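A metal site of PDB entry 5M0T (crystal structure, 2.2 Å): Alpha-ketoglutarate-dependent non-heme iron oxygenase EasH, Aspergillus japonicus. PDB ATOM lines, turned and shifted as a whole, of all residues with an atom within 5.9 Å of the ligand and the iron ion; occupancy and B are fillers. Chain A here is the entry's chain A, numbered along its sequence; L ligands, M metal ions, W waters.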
ATOM      1  N   TYR A  70      18.610  27.204 -18.764  1.00  0.00           N
ATOM      2  CA  TYR A  70      19.302  25.917 -18.497  1.00  0.00           C
ATOM      3  C   TYR A  70      19.985  25.785 -17.110  1.00  0.00           C
ATOM      4  O   TYR A  70      20.167  24.663 -16.621  1.00  0.00           O
ATOM      5  CB  TYR A  70      20.339  25.622 -19.622  1.00  0.00           C
ATOM      6  CG  TYR A  70      19.656  25.308 -20.931  1.00  0.00           C
ATOM      7  CD1 TYR A  70      18.901  24.134 -21.084  1.00  0.00           C
ATOM      8  CD2 TYR A  70      19.706  26.196 -22.001  1.00  0.00           C
ATOM      9  CE1 TYR A  70      18.247  23.849 -22.270  1.00  0.00           C
ATOM     10  CE2 TYR A  70      19.052  25.920 -23.192  1.00  0.00           C
ATOM     11  CZ  TYR A  70      18.306  24.756 -23.329  1.00  0.00           C
ATOM     12  OH  TYR A  70      17.674  24.479 -24.521  1.00  0.00           O
ATOM     13  N   LEU A  71      20.350  26.916 -16.482  1.00  0.00           N
ATOM     14  CA  LEU A  71      21.131  26.921 -15.214  1.00  0.00           C
ATOM     15  C   LEU A  71      20.360  27.226 -13.899  1.00  0.00           C
ATOM     16  O   LEU A  71      20.970  27.242 -12.825  1.00  0.00           O
ATOM     17  CB  LEU A  71      22.337  27.884 -15.338  1.00  0.00           C
ATOM     18  CG  LEU A  71      23.382  27.539 -16.411  1.00  0.00           C
ATOM     19  CD1 LEU A  71      24.352  28.704 -16.610  1.00  0.00           C
ATOM     20  CD2 LEU A  71      24.147  26.265 -16.065  1.00  0.00           C
ATOM     21  N   MET A  74      20.702  25.000 -10.204  1.00  0.00           N
ATOM     22  CA  MET A  74      22.062  24.485 -10.013  1.00  0.00           C
ATOM     23  C   MET A  74      22.843  25.403  -9.096  1.00  0.00           C
ATOM     24  O   MET A  74      22.568  26.613  -9.028  1.00  0.00           O
ATOM     25  CB  MET A  74      22.791  24.409 -11.338  1.00  0.00           C
ATOM     26  CG  MET A  74      22.276  23.322 -12.259  1.00  0.00           C
ATOM     27  SD  MET A  74      23.222  23.259 -13.790  1.00  0.00           S
ATOM     28  CE  MET A  74      23.259  21.484 -14.067  1.00  0.00           C
ATOM     29  N   LEU A 120      29.589  22.885 -11.668  1.00  0.00           N
ATOM     30  CA  LEU A 120      28.139  22.735 -11.565  1.00  0.00           C
ATOM     31  C   LEU A 120      27.775  21.589 -10.609  1.00  0.00           C
ATOM     32  O   LEU A 120      27.954  20.422 -10.951  1.00  0.00           O
ATOM     33  CB  LEU A 120      27.509  22.490 -12.950  1.00  0.00           C
ATOM     34  CG  LEU A 120      27.652  23.570 -14.035  1.00  0.00           C
ATOM     35  CD1 LEU A 120      26.909  23.140 -15.303  1.00  0.00           C
ATOM     36  CD2 LEU A 120      27.168  24.951 -13.600  1.00  0.00           C
ATOM     37  N   GLN A 129      18.249  18.586 -16.796  1.00  0.00           N
ATOM     38  CA  GLN A 129      18.062  19.535 -17.904  1.00  0.00           C
ATOM     39  C   GLN A 129      17.345  18.848 -19.055  1.00  0.00           C
ATOM     40  O   GLN A 129      17.426  17.616 -19.217  1.00  0.00           O
ATOM     41  CB  GLN A 129      19.424  20.028 -18.403  1.00  0.00           C
ATOM     42  CG  GLN A 129      20.151  20.926 -17.442  1.00  0.00           C
ATOM     43  CD  GLN A 129      21.530  21.360 -17.941  1.00  0.00           C
ATOM     44  OE1 GLN A 129      22.270  20.593 -18.541  1.00  0.00           O
ATOM     45  NE2 GLN A 129      21.893  22.607 -17.674  1.00  0.00           N
ATOM     46  N   HIS A 132      19.961  19.441 -25.041  1.00  0.00           N
ATOM     47  CA  HIS A 132      20.233  20.632 -25.850  1.00  0.00           C
ATOM     48  C   HIS A 132      21.611  20.487 -26.521  1.00  0.00           C
ATOM     49  O   HIS A 132      22.427  19.655 -26.108  1.00  0.00           O
ATOM     50  CB  HIS A 132      20.199  21.887 -24.949  1.00  0.00           C
ATOM     51  CG  HIS A 132      21.220  21.865 -23.837  1.00  0.00           C
ATOM     52  ND1 HIS A 132      20.978  21.269 -22.620  1.00  0.00           N
ATOM     53  CD2 HIS A 132      22.488  22.334 -23.788  1.00  0.00           C
ATOM     54  CE1 HIS A 132      22.056  21.394 -21.858  1.00  0.00           C
ATOM     55  NE2 HIS A 132      22.997  22.007 -22.546  1.00  0.00           N
ATOM     56  N   ARG A 133      21.867  21.301 -27.538  1.00  0.00           N
ATOM     57  CA  ARG A 133      23.186  21.389 -28.158  1.00  0.00           C
ATOM     58  C   ARG A 133      23.824  22.676 -27.673  1.00  0.00           C
ATOM     59  O   ARG A 133      23.167  23.721 -27.627  1.00  0.00           O
ATOM     60  CB  ARG A 133      23.055  21.410 -29.680  1.00  0.00           C
ATOM     61  CG  ARG A 133      22.568  20.090 -30.236  1.00  0.00           C
ATOM     62  CD  ARG A 133      22.638  20.045 -31.747  1.00  0.00           C
ATOM     63  NE  ARG A 133      22.294  18.714 -32.225  1.00  0.00           N
ATOM     64  CZ  ARG A 133      21.052  18.263 -32.433  1.00  0.00           C
ATOM     65  NH1 ARG A 133      19.977  19.043 -32.194  1.00  0.00           N
ATOM     66  NH2 ARG A 133      20.875  17.025 -32.872  1.00  0.00           N
ATOM     67  N   GLU A 134      25.106  22.593 -27.318  1.00  0.00           N
ATOM     68  CA  GLU A 134      25.779  23.723 -26.705  1.00  0.00           C
ATOM     69  C   GLU A 134      25.959  24.889 -27.707  1.00  0.00           C
ATOM     70  O   GLU A 134      25.965  26.043 -27.271  1.00  0.00           O
ATOM     71  CB  GLU A 134      27.126  23.307 -26.091  1.00  0.00           C
ATOM     72  CG  GLU A 134      27.380  23.943 -24.706  1.00  0.00           C
ATOM     73  CD  GLU A 134      26.698  23.215 -23.535  1.00  0.00           C
ATOM     74  OE1 GLU A 134      25.466  23.324 -23.355  1.00  0.00           O
ATOM     75  OE2 GLU A 134      27.407  22.505 -22.775  1.00  0.00           O
ATOM     76  N   ASN A 154      33.336  20.822 -25.377  1.00  0.00           N
ATOM     77  CA  ASN A 154      33.130  20.759 -23.928  1.00  0.00           C
ATOM     78  C   ASN A 154      33.877  19.600 -23.284  1.00  0.00           C
ATOM     79  O   ASN A 154      33.551  18.450 -23.527  1.00  0.00           O
ATOM     80  CB  ASN A 154      31.637  20.631 -23.601  1.00  0.00           C
ATOM     81  CG  ASN A 154      31.324  20.922 -22.133  1.00  0.00           C
ATOM     82  OD1 ASN A 154      32.153  20.701 -21.231  1.00  0.00           O
ATOM     83  ND2 ASN A 154      30.121  21.427 -21.884  1.00  0.00           N
ATOM     84  N   LEU A 156      33.927  17.995 -20.032  1.00  0.00           N
ATOM     85  CA  LEU A 156      33.134  17.996 -18.808  1.00  0.00           C
ATOM     86  C   LEU A 156      33.675  16.960 -17.836  1.00  0.00           C
ATOM     87  O   LEU A 156      33.413  15.763 -17.983  1.00  0.00           O
ATOM     88  CB  LEU A 156      31.648  17.784 -19.108  1.00  0.00           C
ATOM     89  CG  LEU A 156      30.689  18.233 -17.980  1.00  0.00           C
ATOM     90  CD1 LEU A 156      29.265  18.429 -18.477  1.00  0.00           C
ATOM     91  CD2 LEU A 156      30.688  17.262 -16.797  1.00  0.00           C
ATOM     92  N   PHE A 162      30.146  10.006 -10.860  1.00  0.00           N
ATOM     93  CA  PHE A 162      29.067  10.297 -11.786  1.00  0.00           C
ATOM     94  C   PHE A 162      28.359   8.969 -12.016  1.00  0.00           C
ATOM     95  O   PHE A 162      28.959   8.049 -12.582  1.00  0.00           O
ATOM     96  CB  PHE A 162      29.633  10.800 -13.130  1.00  0.00           C
ATOM     97  CG  PHE A 162      29.529  12.283 -13.360  1.00  0.00           C
ATOM     98  CD1 PHE A 162      29.770  13.191 -12.333  1.00  0.00           C
ATOM     99  CD2 PHE A 162      29.228  12.766 -14.613  1.00  0.00           C
ATOM    100  CE1 PHE A 162      29.678  14.555 -12.563  1.00  0.00           C
ATOM    101  CE2 PHE A 162      29.154  14.125 -14.851  1.00  0.00           C
ATOM    102  CZ  PHE A 162      29.359  15.031 -13.828  1.00  0.00           C
ATOM    103  N   GLY A 167      22.793  11.775 -11.335  1.00  0.00           N
ATOM    104  CA  GLY A 167      22.659  12.865 -12.311  1.00  0.00           C
ATOM    105  C   GLY A 167      23.769  12.978 -13.348  1.00  0.00           C
ATOM    106  O   GLY A 167      23.911  14.041 -13.985  1.00  0.00           O
ATOM    107  N   ALA A 168      24.522  11.905 -13.569  1.00  0.00           N
ATOM    108  CA  ALA A 168      25.554  11.909 -14.611  1.00  0.00           C
ATOM    109  C   ALA A 168      25.003  12.447 -15.931  1.00  0.00           C
ATOM    110  O   ALA A 168      23.899  12.110 -16.334  1.00  0.00           O
ATOM    111  CB  ALA A 168      26.138  10.509 -14.830  1.00  0.00           C
ATOM    112  N   THR A 169      25.809  13.305 -16.568  1.00  0.00           N
ATOM    113  CA  THR A 169      25.470  13.988 -17.803  1.00  0.00           C
ATOM    114  C   THR A 169      25.018  12.973 -18.834  1.00  0.00           C
ATOM    115  O   THR A 169      25.660  11.954 -19.007  1.00  0.00           O
ATOM    116  CB  THR A 169      26.696  14.749 -18.345  1.00  0.00           C
ATOM    117  OG1 THR A 169      27.231  15.558 -17.304  1.00  0.00           O
ATOM    118  CG2 THR A 169      26.334  15.641 -19.510  1.00  0.00           C
ATOM    119  N   PHE A 204      32.399  16.344 -25.563  1.00  0.00           N
ATOM    120  CA  PHE A 204      31.438  16.463 -26.652  1.00  0.00           C
ATOM    121  C   PHE A 204      31.520  17.813 -27.377  1.00  0.00           C
ATOM    122  O   PHE A 204      31.901  18.815 -26.784  1.00  0.00           O
ATOM    123  CB  PHE A 204      30.012  16.168 -26.196  1.00  0.00           C
ATOM    124  CG  PHE A 204      29.564  16.963 -24.997  1.00  0.00           C
ATOM    125  CD1 PHE A 204      28.947  18.198 -25.159  1.00  0.00           C
ATOM    126  CD2 PHE A 204      29.731  16.469 -23.708  1.00  0.00           C
ATOM    127  CE1 PHE A 204      28.520  18.934 -24.055  1.00  0.00           C
ATOM    128  CE2 PHE A 204      29.308  17.210 -22.597  1.00  0.00           C
ATOM    129  CZ  PHE A 204      28.696  18.428 -22.764  1.00  0.00           C
ATOM    130  N   HIS A 210      22.890  16.792 -25.310  1.00  0.00           N
ATOM    131  CA  HIS A 210      23.295  16.394 -23.975  1.00  0.00           C
ATOM    132  C   HIS A 210      22.484  17.187 -22.937  1.00  0.00           C
ATOM    133  O   HIS A 210      21.836  18.174 -23.270  1.00  0.00           O
ATOM    134  CB  HIS A 210      24.777  16.717 -23.780  1.00  0.00           C
ATOM    135  CG  HIS A 210      25.048  18.178 -23.682  1.00  0.00           C
ATOM    136  ND1 HIS A 210      25.195  18.985 -24.787  1.00  0.00           N
ATOM    137  CD2 HIS A 210      25.082  18.999 -22.608  1.00  0.00           C
ATOM    138  CE1 HIS A 210      25.354  20.229 -24.394  1.00  0.00           C
ATOM    139  NE2 HIS A 210      25.264  20.270 -23.080  1.00  0.00           N
ATOM    140  N   GLY A 211      22.553  16.755 -21.679  1.00  0.00           N
ATOM    141  CA  GLY A 211      22.019  17.535 -20.564  1.00  0.00           C
ATOM    142  C   GLY A 211      22.305  16.877 -19.233  1.00  0.00           C
ATOM    143  O   GLY A 211      22.473  15.664 -19.156  1.00  0.00           O
ATOM    144  N   ALA A 212      22.397  17.688 -18.175  1.00  0.00           N
ATOM    145  CA  ALA A 212      22.609  17.202 -16.813  1.00  0.00           C
ATOM    146  C   ALA A 212      21.456  16.294 -16.449  1.00  0.00           C
ATOM    147  O   ALA A 212      20.312  16.611 -16.768  1.00  0.00           O
ATOM    148  CB  ALA A 212      22.719  18.346 -15.825  1.00  0.00           C
ATOM    149  N   GLY A 213      21.752  15.185 -15.786  1.00  0.00           N
ATOM    150  CA  GLY A 213      20.754  14.181 -15.444  1.00  0.00           C
ATOM    151  C   GLY A 213      20.002  14.540 -14.174  1.00  0.00           C
ATOM    152  O   GLY A 213      20.369  15.473 -13.465  1.00  0.00           O
ATOM    153  N   ARG A 222      26.389  15.950  -6.626  1.00  0.00           N
ATOM    154  CA  ARG A 222      27.097  15.515  -7.848  1.00  0.00           C
ATOM    155  C   ARG A 222      27.773  16.745  -8.477  1.00  0.00           C
ATOM    156  O   ARG A 222      27.092  17.655  -8.915  1.00  0.00           O
ATOM    157  CB  ARG A 222      26.095  14.817  -8.792  1.00  0.00           C
ATOM    158  CG  ARG A 222      26.516  14.536 -10.225  1.00  0.00           C
ATOM    159  CD  ARG A 222      26.497  15.810 -11.054  1.00  0.00           C
ATOM    160  NE  ARG A 222      26.106  15.631 -12.427  1.00  0.00           N
ATOM    161  CZ  ARG A 222      26.084  16.621 -13.316  1.00  0.00           C
ATOM    162  NH1 ARG A 222      26.434  17.880 -13.009  1.00  0.00           N
ATOM    163  NH2 ARG A 222      25.710  16.345 -14.559  1.00  0.00           N
ATOM    164  N   GLY A 224      30.094  18.444 -11.286  1.00  0.00           N
ATOM    165  CA  GLY A 224      30.702  18.390 -12.616  1.00  0.00           C
ATOM    166  C   GLY A 224      31.494  19.644 -12.920  1.00  0.00           C
ATOM    167  O   GLY A 224      31.335  20.661 -12.233  1.00  0.00           O
ATOM    168  N   PRO A 226      32.272  21.549 -16.399  1.00  0.00           N
ATOM    169  CA  PRO A 226      32.317  21.869 -17.815  1.00  0.00           C
ATOM    170  C   PRO A 226      33.392  22.895 -18.124  1.00  0.00           C
ATOM    171  O   PRO A 226      33.491  23.899 -17.455  1.00  0.00           O
ATOM    172  CB  PRO A 226      30.931  22.470 -18.096  1.00  0.00           C
ATOM    173  CG  PRO A 226      30.435  22.908 -16.753  1.00  0.00           C
ATOM    174  CD  PRO A 226      30.940  21.834 -15.842  1.00  0.00           C
ATOM    175  N   ILE A 228      34.532  24.751 -21.621  1.00  0.00           N
ATOM    176  CA  ILE A 228      34.126  24.848 -23.022  1.00  0.00           C
ATOM    177  C   ILE A 228      35.096  25.739 -23.794  1.00  0.00           C
ATOM    178  O   ILE A 228      35.240  26.931 -23.505  1.00  0.00           O
ATOM    179  CB  ILE A 228      32.677  25.334 -23.167  1.00  0.00           C
ATOM    180  CG1 ILE A 228      31.769  24.594 -22.170  1.00  0.00           C
ATOM    181  CG2 ILE A 228      32.191  25.136 -24.589  1.00  0.00           C
ATOM    182  CD1 ILE A 228      30.316  25.008 -22.202  1.00  0.00           C
HETATM  183  C1  LIG L   1      25.017  22.998 -19.795  1.00  0.00           C
HETATM  184  O1  LIG L   1      25.094  23.491 -20.914  1.00  0.00           O
HETATM  185  O2  LIG L   1      24.723  23.674 -18.709  1.00  0.00           O
HETATM  186  C2  LIG L   1      25.292  21.513 -19.509  1.00  0.00           C
HETATM  187  O3  LIG L   1      25.174  20.726 -20.434  1.00  0.00           O
HETATM  188  C3  LIG L   1      25.732  21.047 -18.152  1.00  0.00           C
HETATM  189  C4  LIG L   1      25.799  19.537 -18.041  1.00  0.00           C
HETATM  190  C5  LIG L   1      26.208  19.027 -16.678  1.00  0.00           C
HETATM  191  O4  LIG L   1      26.648  19.918 -15.828  1.00  0.00           O
HETATM  192  O5  LIG L   1      26.124  17.855 -16.406  1.00  0.00           O
HETATM  193 FE    FE M   1      24.878  21.851 -22.113  1.00  0.00          FE
HETATM  194  O   HOH W   1      28.074  22.422 -20.270  1.00  0.00           O
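Of the 23 residues printed, 3 come within 4 Å of the iron ion. Along chain A the residues within 4 Å of the iron ion span positions 132 to 210. The nearest printed residue that does not touch the iron ion is Gln 129 (4.6 Å).
Water W1 lies within hydrogen-bond range of OE2 of Glu 134 (2.6 Å) and ND2 of Asn 154 (2.8 Å).
Leu 71 touches the ligand. CD1 of Leu 120 touches O4 of the ligand (3.3 Å). CD1 of Leu 156 touches C5 of the ligand (3.6 Å). Ala 212 touches the ligand. Hydrophobic or aromatic side chains within 4 Å of the ligand: Leu 71, Leu 120, His 132, Leu 156, His 210 and Ala 212. Within 4 Å of the ligand: Leu 71, Leu 120, Gln 129, His 132, Glu 134, Leu 156, Thr 169, His 210, Ala 212 and Arg 222. The nearest printed residue that does not touch the ligand is Met 74 (4.1 Å).
The iron ion is bound by a ring nitrogen (NE2) of His 210 (1.9 Å), a ring nitrogen (NE2) of His 132 (1.9 Å), the side-chain carboxylate of Glu 134 (2.0 Å), an oxygen (O3) of the ligand (2.0 Å) and an oxygen (O1) of the ligand (2.0 Å). Slightly farther from the iron ion lies the side-chain carboxylate (OE2) of Glu 134 (2.7 Å).
The side-chain amide nitrogen (ND2) of Asn 154 sits at hydrogen-bond distance from the side-chain carboxylate (OE2) of Glu 134. N of Leu 156 is in hydrogen-bond range of OD1 of Asn 154 (3.5 Å). The backbone NH (N) of Leu 120 is in hydrogen-bond range of the backbone carbonyl oxygen (O) of Gly 224 (2.9 Å). The guanidinium group (NH2) of Arg 222 is in hydrogen-bond range of the backbone carbonyl oxygen (O) of Gly 167 (3.0 Å). NE2 of Gln 129 sits at hydrogen-bond distance from O of Tyr 70. The backbone NH (N) of Gln 129 sits at hydrogen-bond distance from the backbone carbonyl oxygen (O) of Ala 212 (2.9 Å). NH2 of Arg 222 lies within hydrogen-bond range of OG1 of Thr 169.
An oxygen (O2) of the ligand is in hydrogen-bond range of the side-chain amide nitrogen (NE2) of Gln 129 (3.2 Å). The guanidinium group (NH2) of Arg 222 lies within salt-bridge range of an oxygen (O5) of the ligand, 2.4 Å away. O5 of the ligand sits at hydrogen-bond distance from OG1 of Thr 169, 2.7 Å away.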
